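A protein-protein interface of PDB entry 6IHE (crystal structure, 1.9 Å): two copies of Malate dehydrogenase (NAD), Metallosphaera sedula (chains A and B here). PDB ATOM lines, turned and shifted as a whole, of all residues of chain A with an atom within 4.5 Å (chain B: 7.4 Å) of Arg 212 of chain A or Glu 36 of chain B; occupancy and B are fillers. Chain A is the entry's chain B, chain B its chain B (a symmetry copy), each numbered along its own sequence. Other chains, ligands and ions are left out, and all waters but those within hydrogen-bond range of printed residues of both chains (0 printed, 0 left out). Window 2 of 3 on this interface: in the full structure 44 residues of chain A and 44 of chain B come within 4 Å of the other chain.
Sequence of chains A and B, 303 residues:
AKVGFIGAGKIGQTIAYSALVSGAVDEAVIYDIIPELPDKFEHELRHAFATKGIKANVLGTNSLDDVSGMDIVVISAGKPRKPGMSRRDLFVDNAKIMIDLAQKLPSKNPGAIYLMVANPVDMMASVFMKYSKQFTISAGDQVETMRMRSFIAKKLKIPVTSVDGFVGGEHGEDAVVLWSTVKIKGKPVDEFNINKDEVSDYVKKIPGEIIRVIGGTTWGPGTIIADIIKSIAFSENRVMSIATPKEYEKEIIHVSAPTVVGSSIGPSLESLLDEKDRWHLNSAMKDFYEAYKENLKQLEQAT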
ATOM      1  N   PRO A  83     -17.503  16.925  21.486  1.00  0.00           N
ATOM      2  CA  PRO A  83     -16.654  17.471  22.554  1.00  0.00           C
ATOM      3  C   PRO A  83     -17.420  17.512  23.858  1.00  0.00           C
ATOM      4  O   PRO A  83     -18.519  18.058  23.925  1.00  0.00           O
ATOM      5  CB  PRO A  83     -16.378  18.892  22.091  1.00  0.00           C
ATOM      6  CG  PRO A  83     -16.275  18.765  20.649  1.00  0.00           C
ATOM      7  CD  PRO A  83     -17.443  17.904  20.316  1.00  0.00           C
ATOM      8  N   GLY A 208      -9.624  13.356  22.166  1.00  0.00           N
ATOM      9  CA  GLY A 208     -10.530  14.457  22.528  1.00  0.00           C
ATOM     10  C   GLY A 208     -10.096  15.778  21.935  1.00  0.00           C
ATOM     11  O   GLY A 208     -10.911  16.553  21.423  1.00  0.00           O
ATOM     12  N   GLU A 209      -8.789  16.004  21.960  1.00  0.00           N
ATOM     13  CA  GLU A 209      -8.195  17.163  21.274  1.00  0.00           C
ATOM     14  C   GLU A 209      -8.362  17.195  19.767  1.00  0.00           C
ATOM     15  O   GLU A 209      -8.731  18.224  19.227  1.00  0.00           O
ATOM     16  CB  GLU A 209      -6.712  17.287  21.633  1.00  0.00           C
ATOM     17  CG  GLU A 209      -6.482  17.674  23.095  1.00  0.00           C
ATOM     18  CD  GLU A 209      -7.011  19.076  23.403  1.00  0.00           C
ATOM     19  OE1 GLU A 209      -8.176  19.236  23.839  1.00  0.00           O
ATOM     20  OE2 GLU A 209      -6.269  20.030  23.132  1.00  0.00           O
ATOM     21  N   ILE A 210      -8.097  16.077  19.089  1.00  0.00           N
ATOM     22  CA  ILE A 210      -8.434  15.964  17.644  1.00  0.00           C
ATOM     23  C   ILE A 210      -9.972  16.159  17.367  1.00  0.00           C
ATOM     24  O   ILE A 210     -10.410  16.815  16.383  1.00  0.00           O
ATOM     25  CB  ILE A 210      -7.954  14.580  17.089  1.00  0.00           C
ATOM     26  CG1 ILE A 210      -6.447  14.395  17.248  1.00  0.00           C
ATOM     27  CG2 ILE A 210      -8.389  14.424  15.626  1.00  0.00           C
ATOM     28  CD1 ILE A 210      -5.982  12.974  17.242  1.00  0.00           C
ATOM     29  N   ILE A 211     -10.821  15.523  18.173  1.00  0.00           N
ATOM     30  CA  ILE A 211     -12.282  15.723  18.043  1.00  0.00           C
ATOM     31  C   ILE A 211     -12.617  17.217  18.216  1.00  0.00           C
ATOM     32  O   ILE A 211     -13.359  17.789  17.417  1.00  0.00           O
ATOM     33  CB  ILE A 211     -13.109  14.904  19.063  1.00  0.00           C
ATOM     34  CG1 ILE A 211     -13.013  13.399  18.774  1.00  0.00           C
ATOM     35  CG2 ILE A 211     -14.593  15.311  19.025  1.00  0.00           C
ATOM     36  CD1 ILE A 211     -13.227  12.551  20.019  1.00  0.00           C
ATOM     37  N   ARG A 212     -12.057  17.853  19.236  1.00  0.00           N
ATOM     38  CA  ARG A 212     -12.262  19.308  19.372  1.00  0.00           C
ATOM     39  C   ARG A 212     -11.850  20.099  18.088  1.00  0.00           C
ATOM     40  O   ARG A 212     -12.617  20.916  17.604  1.00  0.00           O
ATOM     41  CB  ARG A 212     -11.541  19.860  20.596  1.00  0.00           C
ATOM     42  CG  ARG A 212     -11.620  21.373  20.784  1.00  0.00           C
ATOM     43  CD  ARG A 212     -10.942  21.747  22.080  1.00  0.00           C
ATOM     44  NE  ARG A 212      -9.496  21.532  22.073  1.00  0.00           N
ATOM     45  CZ  ARG A 212      -8.589  22.290  21.435  1.00  0.00           C
ATOM     46  NH1 ARG A 212      -8.927  23.353  20.723  1.00  0.00           N
ATOM     47  NH2 ARG A 212      -7.300  21.966  21.478  1.00  0.00           N
ATOM     48  N   VAL A 213     -10.673  19.846  17.519  1.00  0.00           N
ATOM     49  CA  VAL A 213     -10.193  20.726  16.447  1.00  0.00           C
ATOM     50  C   VAL A 213     -10.786  20.313  15.110  1.00  0.00           C
ATOM     51  O   VAL A 213     -11.173  21.152  14.309  1.00  0.00           O
ATOM     52  CB  VAL A 213      -8.644  20.732  16.421  1.00  0.00           C
ATOM     53  CG1 VAL A 213      -8.116  21.587  15.285  1.00  0.00           C
ATOM     54  CG2 VAL A 213      -8.137  21.225  17.752  1.00  0.00           C
ATOM     55  N   ILE A 214     -10.824  19.015  14.835  1.00  0.00           N
ATOM     56  CA  ILE A 214     -11.125  18.542  13.457  1.00  0.00           C
ATOM     57  C   ILE A 214     -12.547  18.082  13.372  1.00  0.00           C
ATOM     58  O   ILE A 214     -13.184  18.201  12.319  1.00  0.00           O
ATOM     59  CB  ILE A 214     -10.137  17.420  13.007  1.00  0.00           C
ATOM     60  CG1 ILE A 214      -8.706  17.933  13.143  1.00  0.00           C
ATOM     61  CG2 ILE A 214     -10.399  16.996  11.559  1.00  0.00           C
ATOM     62  CD1 ILE A 214      -7.631  16.892  12.902  1.00  0.00           C
ATOM     63  N   ASP B  32      -1.986  25.120   7.274  1.00  0.00           N
ATOM     64  CA  ASP B  32      -3.334  25.636   7.130  1.00  0.00           C
ATOM     65  C   ASP B  32      -3.489  26.920   7.983  1.00  0.00           C
ATOM     66  O   ASP B  32      -2.784  27.090   8.990  1.00  0.00           O
ATOM     67  CB  ASP B  32      -4.386  24.554   7.517  1.00  0.00           C
ATOM     68  CG  ASP B  32      -5.788  24.839   6.920  1.00  0.00           C
ATOM     69  OD1 ASP B  32      -6.482  25.787   7.404  1.00  0.00           O
ATOM     70  OD2 ASP B  32      -6.228  24.148   5.966  1.00  0.00           O
ATOM     71  N   ILE B  33      -4.384  27.822   7.563  1.00  0.00           N
ATOM     72  CA  ILE B  33      -4.743  29.039   8.363  1.00  0.00           C
ATOM     73  C   ILE B  33      -5.513  28.717   9.653  1.00  0.00           C
ATOM     74  O   ILE B  33      -5.432  29.465  10.640  1.00  0.00           O
ATOM     75  CB  ILE B  33      -5.535  30.114   7.580  1.00  0.00           C
ATOM     76  CG1 ILE B  33      -6.854  29.555   7.040  1.00  0.00           C
ATOM     77  CG2 ILE B  33      -4.660  30.728   6.485  1.00  0.00           C
ATOM     78  CD1 ILE B  33      -7.612  30.509   6.122  1.00  0.00           C
ATOM     79  N   ILE B  34      -6.239  27.618   9.640  1.00  0.00           N
ATOM     80  CA  ILE B  34      -7.004  27.217  10.789  1.00  0.00           C
ATOM     81  C   ILE B  34      -6.135  26.803  11.957  1.00  0.00           C
ATOM     82  O   ILE B  34      -5.369  25.890  11.892  1.00  0.00           O
ATOM     83  CB  ILE B  34      -8.064  26.207  10.411  1.00  0.00           C
ATOM     84  CG1 ILE B  34      -8.988  26.864   9.410  1.00  0.00           C
ATOM     85  CG2 ILE B  34      -8.820  25.758  11.634  1.00  0.00           C
ATOM     86  CD1 ILE B  34     -10.007  25.973   8.800  1.00  0.00           C
ATOM     87  N   PRO B  35      -6.240  27.531  13.037  1.00  0.00           N
ATOM     88  CA  PRO B  35      -5.414  27.254  14.188  1.00  0.00           C
ATOM     89  C   PRO B  35      -5.566  25.843  14.683  1.00  0.00           C
ATOM     90  O   PRO B  35      -6.646  25.379  14.782  1.00  0.00           O
ATOM     91  CB  PRO B  35      -5.926  28.244  15.217  1.00  0.00           C
ATOM     92  CG  PRO B  35      -6.504  29.323  14.425  1.00  0.00           C
ATOM     93  CD  PRO B  35      -7.156  28.632  13.302  1.00  0.00           C
ATOM     94  N   GLU B  36      -4.453  25.208  14.985  1.00  0.00           N
ATOM     95  CA  GLU B  36      -4.390  23.843  15.487  1.00  0.00           C
ATOM     96  C   GLU B  36      -4.764  22.677  14.577  1.00  0.00           C
ATOM     97  O   GLU B  36      -4.552  21.563  14.925  1.00  0.00           O
ATOM     98  CB  GLU B  36      -5.260  23.700  16.703  1.00  0.00           C
ATOM     99  CG  GLU B  36      -4.779  24.467  17.897  1.00  0.00           C
ATOM    100  CD  GLU B  36      -5.586  24.156  19.114  1.00  0.00           C
ATOM    101  OE1 GLU B  36      -6.540  24.878  19.363  1.00  0.00           O
ATOM    102  OE2 GLU B  36      -5.255  23.183  19.793  1.00  0.00           O
ATOM    103  N   LEU B  37      -5.329  22.968  13.432  1.00  0.00           N
ATOM    104  CA  LEU B  37      -5.739  21.943  12.522  1.00  0.00           C
ATOM    105  C   LEU B  37      -4.516  21.179  12.068  1.00  0.00           C
ATOM    106  O   LEU B  37      -4.454  19.993  12.224  1.00  0.00           O
ATOM    107  CB  LEU B  37      -6.495  22.555  11.339  1.00  0.00           C
ATOM    108  CG  LEU B  37      -6.850  21.717  10.137  1.00  0.00           C
ATOM    109  CD1 LEU B  37      -7.594  20.496  10.567  1.00  0.00           C
ATOM    110  CD2 LEU B  37      -7.668  22.452   9.106  1.00  0.00           C
ATOM    111  N   PRO B  38      -3.525  21.858  11.501  1.00  0.00           N
ATOM    112  CA  PRO B  38      -2.361  21.132  11.030  1.00  0.00           C
ATOM    113  C   PRO B  38      -1.694  20.325  12.097  1.00  0.00           C
ATOM    114  O   PRO B  38      -1.194  19.286  11.818  1.00  0.00           O
ATOM    115  CB  PRO B  38      -1.442  22.238  10.546  1.00  0.00           C
ATOM    116  CG  PRO B  38      -2.377  23.263  10.070  1.00  0.00           C
ATOM    117  CD  PRO B  38      -3.429  23.272  11.125  1.00  0.00           C
ATOM    118  N   ASP B  39      -1.715  20.815  13.308  1.00  0.00           N
ATOM    119  CA  ASP B  39      -1.092  20.135  14.407  1.00  0.00           C
ATOM    120  C   ASP B  39      -1.748  18.806  14.732  1.00  0.00           C
ATOM    121  O   ASP B  39      -1.097  17.840  14.941  1.00  0.00           O
ATOM    122  CB  ASP B  39      -1.151  21.040  15.623  1.00  0.00           C
ATOM    123  CG  ASP B  39      -0.526  20.437  16.828  1.00  0.00           C
ATOM    124  OD1 ASP B  39       0.650  20.130  16.776  1.00  0.00           O
ATOM    125  OD2 ASP B  39      -1.185  20.279  17.845  1.00  0.00           O
ATOM    126  N   LYS B  40      -3.058  18.815  14.779  1.00  0.00           N
ATOM    127  CA  LYS B  40      -3.859  17.643  15.115  1.00  0.00           C
ATOM    128  C   LYS B  40      -3.814  16.616  13.962  1.00  0.00           C
ATOM    129  O   LYS B  40      -3.704  15.451  14.201  1.00  0.00           O
ATOM    130  CB  LYS B  40      -5.278  18.035  15.441  1.00  0.00           C
ATOM    131  CG  LYS B  40      -5.540  18.846  16.702  1.00  0.00           C
ATOM    132  CD  LYS B  40      -4.429  18.920  17.696  1.00  0.00           C
ATOM    133  CE  LYS B  40      -4.874  19.584  18.983  1.00  0.00           C
ATOM    134  NZ  LYS B  40      -3.694  20.219  19.639  1.00  0.00           N
ATOM    135  N   PHE B  41      -3.789  17.067  12.719  1.00  0.00           N
ATOM    136  CA  PHE B  41      -3.560  16.193  11.599  1.00  0.00           C
ATOM    137  C   PHE B  41      -2.214  15.517  11.665  1.00  0.00           C
ATOM    138  O   PHE B  41      -2.085  14.328  11.379  1.00  0.00           O
ATOM    139  CB  PHE B  41      -3.732  16.981  10.300  1.00  0.00           C
ATOM    140  CG  PHE B  41      -3.504  16.179   9.065  1.00  0.00           C
ATOM    141  CD1 PHE B  41      -4.089  14.904   8.908  1.00  0.00           C
ATOM    142  CD2 PHE B  41      -2.773  16.715   8.000  1.00  0.00           C
ATOM    143  CE1 PHE B  41      -3.907  14.197   7.728  1.00  0.00           C
ATOM    144  CE2 PHE B  41      -2.577  16.003   6.828  1.00  0.00           C
ATOM    145  CZ  PHE B  41      -3.158  14.753   6.678  1.00  0.00           C
ATOM    146  N   GLU B  42      -1.177  16.252  12.088  1.00  0.00           N
ATOM    147  CA  GLU B  42       0.126  15.693  12.253  1.00  0.00           C
ATOM    148  C   GLU B  42       0.064  14.557  13.246  1.00  0.00           C
ATOM    149  O   GLU B  42       0.726  13.532  13.021  1.00  0.00           O
ATOM    150  CB  GLU B  42       1.213  16.732  12.697  1.00  0.00           C
ATOM    151  CG  GLU B  42       2.543  16.144  13.207  1.00  0.00           C
ATOM    152  CD  GLU B  42       3.479  17.145  13.908  1.00  0.00           C
ATOM    153  OE1 GLU B  42       3.459  18.360  13.578  1.00  0.00           O
ATOM    154  OE2 GLU B  42       4.318  16.664  14.681  1.00  0.00           O
ATOM    155  N   THR B  61       1.871  22.774  10.718  1.00  0.00           N
ATOM    156  CA  THR B  61       2.151  24.101  11.173  1.00  0.00           C
ATOM    157  C   THR B  61       1.201  25.224  10.803  1.00  0.00           C
ATOM    158  O   THR B  61       0.599  25.207   9.767  1.00  0.00           O
ATOM    159  CB  THR B  61       3.541  24.451  10.642  1.00  0.00           C
ATOM    160  OG1 THR B  61       3.935  25.727  11.101  1.00  0.00           O
ATOM    161  CG2 THR B  61       3.547  24.445   9.136  1.00  0.00           C
ATOM    162  N   ASN B  62       1.106  26.217  11.683  1.00  0.00           N
ATOM    163  CA  ASN B  62       0.312  27.400  11.398  1.00  0.00           C
ATOM    164  C   ASN B  62       1.227  28.559  10.929  1.00  0.00           C
ATOM    165  O   ASN B  62       0.753  29.644  10.682  1.00  0.00           O
ATOM    166  CB  ASN B  62      -0.573  27.842  12.554  1.00  0.00           C
ATOM    167  CG  ASN B  62      -1.797  26.987  12.721  1.00  0.00           C
ATOM    168  OD1 ASN B  62      -1.997  26.420  13.750  1.00  0.00           O
ATOM    169  ND2 ASN B  62      -2.627  26.928  11.713  1.00  0.00           N
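NH2 of Arg 212 of chain A lies within salt-bridge range of OE2 of Glu 36 of chain B (2.9 Å).
The side-chain amide oxygen (OD1) of Asn 62 of chain B is in hydrogen-bond range of the backbone NH (N) of Glu 36 of chain B. OD2 of Asp 39 of chain B lies within salt-bridge range of NZ of Lys 40 of chain B, at 3.1 Å. The side-chain amino group of Lys 40 of chain B lies within salt-bridge range of the side-chain carboxylate of Glu 36 of chain B, 3.4 Å away. The side-chain carboxylate of Glu 209 of chain A lies within salt-bridge range of the guanidinium group of Arg 212 of chain A (2.7 Å).
Glu 209 of chain A touches Lys 40 of chain B (CB to CE, 3.96 Å). CG1 of Val 213 of chain A touches O of Glu 36 of chain B, at 3.6 Å. Leu 37 of chain B touches Val 213 of chain A. Val 213 of chain A touches Lys 40 of chain B. Ile 214 of chain A touches Leu 37 of chain B. CD1 of Ile 214 of chain A touches CB of Lys 40 of chain B (3.6 Å). Ile 214 of chain A touches Phe 41 of chain B (CD1 to N, 3.9 Å).
Of chain B, only Glu 36 comes within 4 Å of Arg 212 of chain A. Of chain A, only Arg 212 (2.9 Å) and Val 213 (3.6 Å) come within 4 Å of Glu 36 of chain B. Of the printed residues of chain B, Glu 209 of chain A touches Lys 40 (3.96 Å). Printed residues of chain A within 4 Å of Lys 40 of chain B: Glu 209, Val 213 and Ile 214. The nearest printed residue of chain A that does not touch Leu 37 of chain B is Ile 210 of chain A (7.4 Å).
Hydrophobic or aromatic side chains of chain A that line the printed part of chain B: Val 213 and Ile 214. Hydrophobic or aromatic side chains of chain B within 4 Å of the printed part of chain A: Leu 37.
No position is printed for both chains. Of the 8 pairs that touch across the chains among the printed residues, none has its exchanged pair printed and touching as well.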
